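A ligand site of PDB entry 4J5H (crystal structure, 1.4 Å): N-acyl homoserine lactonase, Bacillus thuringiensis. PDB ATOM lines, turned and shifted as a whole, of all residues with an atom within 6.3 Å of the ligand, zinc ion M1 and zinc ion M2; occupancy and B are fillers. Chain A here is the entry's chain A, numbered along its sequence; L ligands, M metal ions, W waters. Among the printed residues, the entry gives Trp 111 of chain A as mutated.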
ATOM      1  N   CYS A  18       8.363  30.760  22.540  1.00  0.00           N
ATOM      2  CA  CYS A  18       8.601  30.036  23.767  1.00  0.00           C
ATOM      3  C   CYS A  18       8.997  28.608  23.456  1.00  0.00           C
ATOM      4  O   CYS A  18       8.472  27.991  22.535  1.00  0.00           O
ATOM      5  CB  CYS A  18       7.405  30.088  24.717  1.00  0.00           C
ATOM      6  SG  CYS A  18       5.891  29.334  24.099  1.00  0.00           S
ATOM      7  N   MET A  19       9.946  28.112  24.255  1.00  0.00           N
ATOM      8  CA  MET A  19      10.357  26.731  24.167  1.00  0.00           C
ATOM      9  C   MET A  19       9.394  25.942  25.003  1.00  0.00           C
ATOM     10  O   MET A  19       9.075  26.322  26.130  1.00  0.00           O
ATOM     11  CB  MET A  19      11.741  26.487  24.756  1.00  0.00           C
ATOM     12  CG  MET A  19      12.826  27.377  24.222  1.00  0.00           C
ATOM     13  SD  MET A  19      13.111  27.279  22.428  1.00  0.00           S
ATOM     14  CE  MET A  19      13.442  25.538  22.251  1.00  0.00           C
ATOM     15  N   LEU A  20       8.940  24.832  24.443  1.00  0.00           N
ATOM     16  CA  LEU A  20       8.008  23.935  25.087  1.00  0.00           C
ATOM     17  C   LEU A  20       8.425  22.499  24.797  1.00  0.00           C
ATOM     18  O   LEU A  20       8.707  22.132  23.653  1.00  0.00           O
ATOM     19  CB  LEU A  20       6.583  24.154  24.569  1.00  0.00           C
ATOM     20  CG  LEU A  20       5.475  23.302  25.168  1.00  0.00           C
ATOM     21  CD1 LEU A  20       5.380  23.476  26.671  1.00  0.00           C
ATOM     22  CD2 LEU A  20       4.152  23.677  24.493  1.00  0.00           C
ATOM     23  N   LEU A  37       8.432  27.482  19.738  1.00  0.00           N
ATOM     24  CA  LEU A  37       7.097  27.700  19.182  1.00  0.00           C
ATOM     25  C   LEU A  37       6.783  29.166  19.102  1.00  0.00           C
ATOM     26  O   LEU A  37       7.259  29.934  19.943  1.00  0.00           O
ATOM     27  CB  LEU A  37       6.050  27.078  20.085  1.00  0.00           C
ATOM     28  CG  LEU A  37       6.112  25.580  20.285  1.00  0.00           C
ATOM     29  CD1 LEU A  37       4.984  25.189  21.223  1.00  0.00           C
ATOM     30  CD2 LEU A  37       6.019  24.888  18.955  1.00  0.00           C
ATOM     31  N   PHE A  68      10.610  30.246  34.721  1.00  0.00           N
ATOM     32  CA  PHE A  68       9.877  29.180  35.403  1.00  0.00           C
ATOM     33  C   PHE A  68      10.759  28.250  36.207  1.00  0.00           C
ATOM     34  O   PHE A  68      10.323  27.190  36.668  1.00  0.00           O
ATOM     35  CB  PHE A  68       9.008  28.422  34.412  1.00  0.00           C
ATOM     36  CG  PHE A  68       7.940  29.282  33.824  1.00  0.00           C
ATOM     37  CD1 PHE A  68       7.023  29.955  34.627  1.00  0.00           C
ATOM     38  CD2 PHE A  68       7.900  29.492  32.458  1.00  0.00           C
ATOM     39  CE1 PHE A  68       6.057  30.798  34.051  1.00  0.00           C
ATOM     40  CE2 PHE A  68       6.922  30.321  31.899  1.00  0.00           C
ATOM     41  CZ  PHE A  68       6.021  30.976  32.688  1.00  0.00           C
ATOM     42  N   THR A  71       9.535  26.225  39.637  1.00  0.00           N
ATOM     43  CA  THR A  71       8.100  25.966  39.509  1.00  0.00           C
ATOM     44  C   THR A  71       7.886  24.574  38.953  1.00  0.00           C
ATOM     45  O   THR A  71       8.847  23.907  38.529  1.00  0.00           O
ATOM     46  CB  THR A  71       7.420  26.935  38.520  1.00  0.00           C
ATOM     47  OG1 THR A  71       7.741  26.563  37.175  1.00  0.00           O
ATOM     48  CG2 THR A  71       7.852  28.381  38.777  1.00  0.00           C
ATOM     49  N   PHE A  72       6.626  24.157  38.906  1.00  0.00           N
ATOM     50  CA  PHE A  72       6.270  22.821  38.439  1.00  0.00           C
ATOM     51  C   PHE A  72       6.541  22.592  36.938  1.00  0.00           C
ATOM     52  O   PHE A  72       6.484  21.462  36.475  1.00  0.00           O
ATOM     53  CB  PHE A  72       4.811  22.465  38.817  1.00  0.00           C
ATOM     54  CG  PHE A  72       3.761  23.248  38.053  1.00  0.00           C
ATOM     55  CD1 PHE A  72       3.431  24.544  38.440  1.00  0.00           C
ATOM     56  CD2 PHE A  72       3.088  22.663  36.979  1.00  0.00           C
ATOM     57  CE1 PHE A  72       2.471  25.257  37.728  1.00  0.00           C
ATOM     58  CE2 PHE A  72       2.120  23.385  36.275  1.00  0.00           C
ATOM     59  CZ  PHE A  72       1.818  24.680  36.652  1.00  0.00           C
ATOM     60  N   VAL A  73       6.865  23.658  36.187  1.00  0.00           N
ATOM     61  CA  VAL A  73       7.218  23.530  34.762  1.00  0.00           C
ATOM     62  C   VAL A  73       8.691  23.883  34.445  1.00  0.00           C
ATOM     63  O   VAL A  73       9.040  24.065  33.261  1.00  0.00           O
ATOM     64  CB  VAL A  73       6.266  24.355  33.887  1.00  0.00           C
ATOM     65  CG1 VAL A  73       4.818  23.982  34.172  1.00  0.00           C
ATOM     66  CG2 VAL A  73       6.473  25.845  34.099  1.00  0.00           C
ATOM     67  N   ILE A  77       9.179  24.835  29.949  1.00  0.00           N
ATOM     68  CA  ILE A  77       8.708  26.068  29.305  1.00  0.00           C
ATOM     69  C   ILE A  77       9.771  27.131  29.521  1.00  0.00           C
ATOM     70  O   ILE A  77      10.093  27.451  30.678  1.00  0.00           O
ATOM     71  CB  ILE A  77       7.372  26.571  29.909  1.00  0.00           C
ATOM     72  CG1 ILE A  77       6.277  25.502  29.778  1.00  0.00           C
ATOM     73  CG2 ILE A  77       6.966  27.861  29.237  1.00  0.00           C
ATOM     74  CD1 ILE A  77       4.903  25.909  30.280  1.00  0.00           C
ATOM     75  N   HIS A 108      -7.776  33.171  26.422  1.00  0.00           N
ATOM     76  CA  HIS A 108      -7.664  32.628  27.709  1.00  0.00           C
ATOM     77  C   HIS A 108      -6.552  33.382  28.446  1.00  0.00           C
ATOM     78  O   HIS A 108      -5.905  34.263  27.863  1.00  0.00           O
ATOM     79  CB  HIS A 108      -7.465  31.114  27.663  1.00  0.00           C
ATOM     80  CG  HIS A 108      -6.207  30.614  27.037  1.00  0.00           C
ATOM     81  ND1 HIS A 108      -5.744  30.991  25.788  1.00  0.00           N
ATOM     82  CD2 HIS A 108      -5.382  29.639  27.457  1.00  0.00           C
ATOM     83  CE1 HIS A 108      -4.680  30.264  25.487  1.00  0.00           C
ATOM     84  NE2 HIS A 108      -4.441  29.444  26.487  1.00  0.00           N
ATOM     85  N   HIS A 110      -3.761  32.102  30.092  1.00  0.00           N
ATOM     86  CA  HIS A 110      -2.415  31.562  30.149  1.00  0.00           C
ATOM     87  C   HIS A 110      -1.361  32.634  29.880  1.00  0.00           C
ATOM     88  O   HIS A 110      -1.633  33.628  29.220  1.00  0.00           O
ATOM     89  CB  HIS A 110      -2.248  30.360  29.218  1.00  0.00           C
ATOM     90  CG  HIS A 110      -2.950  29.127  29.700  1.00  0.00           C
ATOM     91  ND1 HIS A 110      -3.190  28.046  28.883  1.00  0.00           N
ATOM     92  CD2 HIS A 110      -3.438  28.799  30.915  1.00  0.00           C
ATOM     93  CE1 HIS A 110      -3.808  27.105  29.590  1.00  0.00           C
ATOM     94  NE2 HIS A 110      -3.995  27.545  30.817  1.00  0.00           N
ATOM     95  N   TRP A 111      -0.169  32.375  30.396  1.00  0.00           N
ATOM     96  CA  TRP A 111       0.878  33.379  30.584  1.00  0.00           C
ATOM     97  C   TRP A 111       1.334  34.059  29.302  1.00  0.00           C
ATOM     98  O   TRP A 111       1.738  35.213  29.315  1.00  0.00           O
ATOM     99  CB  TRP A 111       2.059  32.761  31.368  1.00  0.00           C
ATOM    100  CG  TRP A 111       2.860  31.832  30.510  1.00  0.00           C
ATOM    101  CD1 TRP A 111       2.550  30.544  30.160  1.00  0.00           C
ATOM    102  CD2 TRP A 111       4.034  32.171  29.791  1.00  0.00           C
ATOM    103  NE1 TRP A 111       3.483  30.052  29.283  1.00  0.00           N
ATOM    104  CE2 TRP A 111       4.411  31.027  29.038  1.00  0.00           C
ATOM    105  CE3 TRP A 111       4.838  33.321  29.727  1.00  0.00           C
ATOM    106  CZ2 TRP A 111       5.543  31.011  28.222  1.00  0.00           C
ATOM    107  CZ3 TRP A 111       5.965  33.283  28.921  1.00  0.00           C
ATOM    108  CH2 TRP A 111       6.293  32.139  28.169  1.00  0.00           C
ATOM    109  N   ASP A 112       1.305  33.314  28.208  1.00  0.00           N
ATOM    110  CA  ASP A 112       1.755  33.775  26.907  1.00  0.00           C
ATOM    111  C   ASP A 112       0.631  34.332  26.041  1.00  0.00           C
ATOM    112  O   ASP A 112       0.866  34.703  24.878  1.00  0.00           O
ATOM    113  CB  ASP A 112       2.570  32.719  26.157  1.00  0.00           C
ATOM    114  CG  ASP A 112       1.799  31.435  25.912  1.00  0.00           C
ATOM    115  OD1 ASP A 112       0.981  31.004  26.745  1.00  0.00           O
ATOM    116  OD2 ASP A 112       2.057  30.812  24.874  1.00  0.00           O
ATOM    117  N   HIS A 113      -0.560  34.392  26.622  1.00  0.00           N
ATOM    118  CA  HIS A 113      -1.748  34.960  25.979  1.00  0.00           C
ATOM    119  C   HIS A 113      -2.305  36.211  26.672  1.00  0.00           C
ATOM    120  O   HIS A 113      -2.908  37.063  26.003  1.00  0.00           O
ATOM    121  CB  HIS A 113      -2.847  33.927  25.867  1.00  0.00           C
ATOM    122  CG  HIS A 113      -2.479  32.815  24.978  1.00  0.00           C
ATOM    123  ND1 HIS A 113      -2.777  32.812  23.636  1.00  0.00           N
ATOM    124  CD2 HIS A 113      -1.799  31.679  25.230  1.00  0.00           C
ATOM    125  CE1 HIS A 113      -2.255  31.727  23.098  1.00  0.00           C
ATOM    126  NE2 HIS A 113      -1.690  31.012  24.052  1.00  0.00           N
ATOM    127  N   GLU A 139      -3.044  27.040  39.813  1.00  0.00           N
ATOM    128  CA  GLU A 139      -1.601  27.292  39.900  1.00  0.00           C
ATOM    129  C   GLU A 139      -0.930  27.657  38.578  1.00  0.00           C
ATOM    130  O   GLU A 139       0.138  28.236  38.580  1.00  0.00           O
ATOM    131  CB  GLU A 139      -0.864  26.107  40.517  1.00  0.00           C
ATOM    132  CG  GLU A 139      -0.921  24.829  39.699  1.00  0.00           C
ATOM    133  CD  GLU A 139      -0.363  23.617  40.456  1.00  0.00           C
ATOM    134  OE1 GLU A 139      -0.458  22.489  39.934  1.00  0.00           O
ATOM    135  OE2 GLU A 139       0.166  23.810  41.577  1.00  0.00           O
ATOM    136  N   GLU A 140      -1.542  27.281  37.460  1.00  0.00           N
ATOM    137  CA  GLU A 140      -0.953  27.566  36.148  1.00  0.00           C
ATOM    138  C   GLU A 140      -1.156  29.017  35.680  1.00  0.00           C
ATOM    139  O   GLU A 140      -0.806  29.357  34.547  1.00  0.00           O
ATOM    140  CB  GLU A 140      -1.436  26.564  35.082  1.00  0.00           C
ATOM    141  CG  GLU A 140      -2.901  26.642  34.670  1.00  0.00           C
ATOM    142  CD  GLU A 140      -3.847  25.818  35.513  1.00  0.00           C
ATOM    143  OE1 GLU A 140      -4.979  25.563  35.037  1.00  0.00           O
ATOM    144  OE2 GLU A 140      -3.479  25.391  36.646  1.00  0.00           O
ATOM    145  N   TYR A 141      -1.758  29.856  36.529  1.00  0.00           N
ATOM    146  CA  TYR A 141      -1.964  31.270  36.203  1.00  0.00           C
ATOM    147  C   TYR A 141      -1.023  32.195  36.948  1.00  0.00           C
ATOM    148  O   TYR A 141      -0.885  32.103  38.189  1.00  0.00           O
ATOM    149  CB  TYR A 141      -3.406  31.680  36.458  1.00  0.00           C
ATOM    150  CG  TYR A 141      -4.356  30.968  35.485  1.00  0.00           C
ATOM    151  CD1 TYR A 141      -4.603  31.504  34.238  1.00  0.00           C
ATOM    152  CD2 TYR A 141      -4.929  29.735  35.804  1.00  0.00           C
ATOM    153  CE1 TYR A 141      -5.425  30.861  33.362  1.00  0.00           C
ATOM    154  CE2 TYR A 141      -5.772  29.083  34.931  1.00  0.00           C
ATOM    155  CZ  TYR A 141      -6.039  29.674  33.718  1.00  0.00           C
ATOM    156  OH  TYR A 141      -6.837  29.043  32.798  1.00  0.00           O
ATOM    157  N   MET A 142      -0.358  33.054  36.177  1.00  0.00           N
ATOM    158  CA  MET A 142       0.553  34.046  36.732  1.00  0.00           C
ATOM    159  C   MET A 142      -0.243  35.255  37.180  1.00  0.00           C
ATOM    160  O   MET A 142      -1.248  35.594  36.547  1.00  0.00           O
ATOM    161  CB  MET A 142       1.574  34.484  35.670  1.00  0.00           C
ATOM    162  CG  MET A 142       2.529  33.407  35.189  1.00  0.00           C
ATOM    163  SD  MET A 142       3.824  34.064  34.142  1.00  0.00           S
ATOM    164  CE  MET A 142       4.874  34.976  35.251  1.00  0.00           C
ATOM    165  N   HIS A 173      -8.794  22.999  27.039  1.00  0.00           N
ATOM    166  CA  HIS A 173      -7.399  23.329  27.169  1.00  0.00           C
ATOM    167  C   HIS A 173      -7.180  24.177  28.430  1.00  0.00           C
ATOM    168  O   HIS A 173      -6.178  24.005  29.167  1.00  0.00           O
ATOM    169  CB  HIS A 173      -6.869  24.028  25.918  1.00  0.00           C
ATOM    170  CG  HIS A 173      -5.563  24.696  26.131  1.00  0.00           C
ATOM    171  ND1 HIS A 173      -4.356  24.015  26.240  1.00  0.00           N
ATOM    172  CD2 HIS A 173      -5.295  25.998  26.331  1.00  0.00           C
ATOM    173  CE1 HIS A 173      -3.403  24.891  26.500  1.00  0.00           C
ATOM    174  NE2 HIS A 173      -3.950  26.097  26.533  1.00  0.00           N
ATOM    175  N   SER A 174      -8.102  25.147  28.623  1.00  0.00           N
ATOM    176  CA  SER A 174      -8.239  25.874  29.874  1.00  0.00           C
ATOM    177  C   SER A 174      -9.718  25.945  30.199  1.00  0.00           C
ATOM    178  O   SER A 174     -10.543  25.666  29.344  1.00  0.00           O
ATOM    179  CB  SER A 174      -7.639  27.256  29.759  1.00  0.00           C
ATOM    180  OG  SER A 174      -8.407  28.117  28.919  1.00  0.00           O
ATOM    181  N   HIS A 177     -11.486  28.625  27.813  1.00  0.00           N
ATOM    182  CA  HIS A 177     -10.860  28.952  26.560  1.00  0.00           C
ATOM    183  C   HIS A 177     -11.930  29.304  25.516  1.00  0.00           C
ATOM    184  O   HIS A 177     -12.982  28.661  25.446  1.00  0.00           O
ATOM    185  CB  HIS A 177     -10.011  27.769  26.069  1.00  0.00           C
ATOM    186  CG  HIS A 177      -9.241  28.064  24.835  1.00  0.00           C
ATOM    187  ND1 HIS A 177      -9.788  27.988  23.573  1.00  0.00           N
ATOM    188  CD2 HIS A 177      -7.996  28.553  24.677  1.00  0.00           C
ATOM    189  CE1 HIS A 177      -8.901  28.395  22.694  1.00  0.00           C
ATOM    190  NE2 HIS A 177      -7.799  28.745  23.350  1.00  0.00           N
ATOM    191  N   ILE A 194      -6.910  29.185  18.312  1.00  0.00           N
ATOM    192  CA  ILE A 194      -6.016  29.458  19.448  1.00  0.00           C
ATOM    193  C   ILE A 194      -5.615  28.131  20.064  1.00  0.00           C
ATOM    194  O   ILE A 194      -5.282  27.215  19.318  1.00  0.00           O
ATOM    195  CB  ILE A 194      -6.567  30.520  20.433  1.00  0.00           C
ATOM    196  CG1 ILE A 194      -7.362  31.608  19.706  1.00  0.00           C
ATOM    197  CG2 ILE A 194      -5.410  31.110  21.248  1.00  0.00           C
ATOM    198  CD1 ILE A 194      -6.537  32.549  18.882  1.00  0.00           C
ATOM    199  N   ASP A 195      -5.640  27.992  21.377  1.00  0.00           N
ATOM    200  CA  ASP A 195      -5.148  26.790  22.018  1.00  0.00           C
ATOM    201  C   ASP A 195      -6.217  25.684  22.162  1.00  0.00           C
ATOM    202  O   ASP A 195      -5.981  24.704  22.860  1.00  0.00           O
ATOM    203  CB  ASP A 195      -4.535  27.111  23.379  1.00  0.00           C
ATOM    204  CG  ASP A 195      -3.210  27.865  23.292  1.00  0.00           C
ATOM    205  OD1 ASP A 195      -2.790  28.210  22.189  1.00  0.00           O
ATOM    206  OD2 ASP A 195      -2.603  28.138  24.357  1.00  0.00           O
ATOM    207  N   TYR A 198      -3.098  23.245  19.487  1.00  0.00           N
ATOM    208  CA  TYR A 198      -1.792  23.834  19.255  1.00  0.00           C
ATOM    209  C   TYR A 198      -1.365  23.655  17.809  1.00  0.00           C
ATOM    210  O   TYR A 198      -0.820  24.563  17.203  1.00  0.00           O
ATOM    211  CB  TYR A 198      -0.728  23.210  20.151  1.00  0.00           C
ATOM    212  CG  TYR A 198      -0.697  23.566  21.606  1.00  0.00           C
ATOM    213  CD1 TYR A 198      -1.456  24.599  22.141  1.00  0.00           C
ATOM    214  CD2 TYR A 198       0.158  22.893  22.456  1.00  0.00           C
ATOM    215  CE1 TYR A 198      -1.349  24.929  23.477  1.00  0.00           C
ATOM    216  CE2 TYR A 198       0.285  23.210  23.791  1.00  0.00           C
ATOM    217  CZ  TYR A 198      -0.470  24.228  24.306  1.00  0.00           C
ATOM    218  OH  TYR A 198      -0.350  24.554  25.648  1.00  0.00           O
ATOM    219  N   ALA A 210      -1.355  19.295  25.772  1.00  0.00           N
ATOM    220  CA  ALA A 210      -1.512  19.780  27.130  1.00  0.00           C
ATOM    221  C   ALA A 210      -2.839  20.496  27.317  1.00  0.00           C
ATOM    222  O   ALA A 210      -3.227  21.365  26.490  1.00  0.00           O
ATOM    223  CB  ALA A 210      -0.383  20.703  27.488  1.00  0.00           C
ATOM    224  N   GLY A 238      -2.885  27.257  17.154  1.00  0.00           N
ATOM    225  CA  GLY A 238      -2.313  28.138  18.197  1.00  0.00           C
ATOM    226  C   GLY A 238      -0.810  28.300  18.259  1.00  0.00           C
ATOM    227  O   GLY A 238      -0.285  29.409  18.478  1.00  0.00           O
ATOM    228  N   HIS A 239      -0.105  27.188  18.074  1.00  0.00           N
ATOM    229  CA  HIS A 239       1.386  27.163  18.179  1.00  0.00           C
ATOM    230  C   HIS A 239       1.929  26.107  17.234  1.00  0.00           C
ATOM    231  O   HIS A 239       2.407  25.035  17.680  1.00  0.00           O
ATOM    232  CB  HIS A 239       1.848  26.855  19.600  1.00  0.00           C
ATOM    233  CG  HIS A 239       1.326  27.798  20.645  1.00  0.00           C
ATOM    234  ND1 HIS A 239       1.830  29.067  20.818  1.00  0.00           N
ATOM    235  CD2 HIS A 239       0.358  27.660  21.591  1.00  0.00           C
ATOM    236  CE1 HIS A 239       1.212  29.664  21.820  1.00  0.00           C
ATOM    237  NE2 HIS A 239       0.299  28.838  22.296  1.00  0.00           N
HETATM  238  O1  LIG L   1      -1.136  27.765  26.830  1.00  0.00           O
HETATM  239  C1  LIG L   1      -0.045  28.139  26.378  1.00  0.00           C
HETATM  240  O2  LIG L   1      -0.004  28.821  25.297  1.00  0.00           O
HETATM  241  C2  LIG L   1       1.202  27.748  27.141  1.00  0.00           C
HETATM  242  C3  LIG L   1       2.149  27.113  26.099  1.00  0.00           C
HETATM  243  C4  LIG L   1       3.586  26.995  26.543  1.00  0.00           C
HETATM  244  O3  LIG L   1       4.048  28.280  26.970  1.00  0.00           O
HETATM  245  N1  LIG L   1       0.951  26.720  28.162  1.00  0.00           N
HETATM  246  C5  LIG L   1       0.485  27.093  29.357  1.00  0.00           C
HETATM  247  O4  LIG L   1       0.309  28.271  29.705  1.00  0.00           O
HETATM  248  C6  LIG L   1       0.184  25.997  30.326  1.00  0.00           C
HETATM  249  C7  LIG L   1       0.428  26.393  31.774  1.00  0.00           C
HETATM  250  C8  LIG L   1       1.908  26.649  31.998  1.00  0.00           C
HETATM  251  C9  LIG L   1       2.241  26.867  33.469  1.00  0.00           C
HETATM  252  C10 LIG L   1       2.718  28.273  33.757  1.00  0.00           C
HETATM  253  C11 LIG L   1       3.271  28.323  35.186  1.00  0.00           C
HETATM  254  C12 LIG L   1       2.723  29.526  35.950  1.00  0.00           C
HETATM  255  C13 LIG L   1       3.588  29.958  37.145  1.00  0.00           C
HETATM  256  C14 LIG L   1       4.058  28.807  38.004  1.00  0.00           C
HETATM  257 ZN    ZN M   1      -0.984  29.129  23.835  1.00  0.00          ZN
HETATM  258 ZN    ZN M   2      -3.023  27.925  26.733  1.00  0.00          ZN
HETATM  259  O   HOH W   1      -0.313  29.922  31.995  1.00  0.00           O
HETATM  260  O   HOH W   2       1.644  23.543  27.561  1.00  0.00           O
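Water W1 lies within hydrogen-bond range of the backbone carbonyl oxygen (O) of Glu 140 (2.7 Å), an oxygen (O4) of the ligand (2.9 Å) and the backbone NH (N) of Trp 111 (2.9 Å).
Water W2 bridges the side-chain hydroxyl (OH) of Tyr 198 (2.9 Å) and a nitrogen (N1) of the ligand (3.3 Å).
N of Asp 195 is in hydrogen-bond range of NE2 of His 177, 3.0 Å away.
The backbone carbonyl oxygen of Tyr 198 lies within hydrogen-bond range of the backbone NH of His 239.
O of Ala 210 sits at hydrogen-bond distance from ND1 of His 173 (2.9 Å).
N of Gly 238 sits at hydrogen-bond distance from O of Tyr 198, at 3.4 Å.
The backbone carbonyl oxygen of Cys 18 is in hydrogen-bond range of the backbone NH of Leu 37.
The backbone carbonyl oxygen (O) of Phe 68 is in hydrogen-bond range of the side-chain hydroxyl (OG1) of Thr 71.
The side-chain hydroxyl (OG1) of Thr 71 sits close to the backbone NH (N) of Val 73, 3.2 Å away.
Residues that only touch zinc ion M1: Asp 112.
The nearest printed residue that does not touch zinc ion M1 is His 108 (4.2 Å).
An oxygen (O2) of the ligand lies close to the side-chain carboxylate (OD1) of Asp 112 (2.8 Å).
Leu 20 touches the ligand.
Phe 68 touches the ligand (CE1 to C11, 3.9 Å).
Thr 71 touches the ligand.
Phe 72 touches the ligand.
Val 73 touches the ligand (CG1 to C9, 3.9 Å).
Ile 77 touches the ligand.
Glu 139 touches the ligand (O to C12, 3.9 Å).
O of Glu 140 touches C10 of the ligand, at 3.8 Å.
Met 142 touches the ligand (CG to C12, 3.96 Å).
Tyr 198 touches the ligand.
Hydrophobic or aromatic side chains that line the ligand: Leu 20, Phe 68, Phe 72, Val 73, Ile 77, His 110, Trp 111, His 113, Met 142, His 173 and His 239.
The nearest printed residue that does not touch the ligand is Tyr 141 (4.5 Å).
The indole nitrogen of Trp 111 sits at hydrogen-bond distance from an oxygen (O3) of the ligand, 3.0 Å away.
SG of Cys 18 sits at hydrogen-bond distance from O3 of the ligand (3.6 Å).
Zinc ion M1 is bound by O2 of the ligand, OD2 of Asp 195, NE2 of His 113 and NE2 of His 239.
Slightly farther from zinc ion M1 lies OD1 of Asp 195 (2.6 Å).
Zinc ion M2 is bound by an oxygen (O1) of the ligand (1.9 Å), a ring nitrogen (NE2) of His 173 (2.1 Å), a ring nitrogen (NE2) of His 108 (2.1 Å), a ring nitrogen (ND1) of His 110 (2.2 Å) and the side-chain carboxylate of Asp 195 (2.4 Å).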
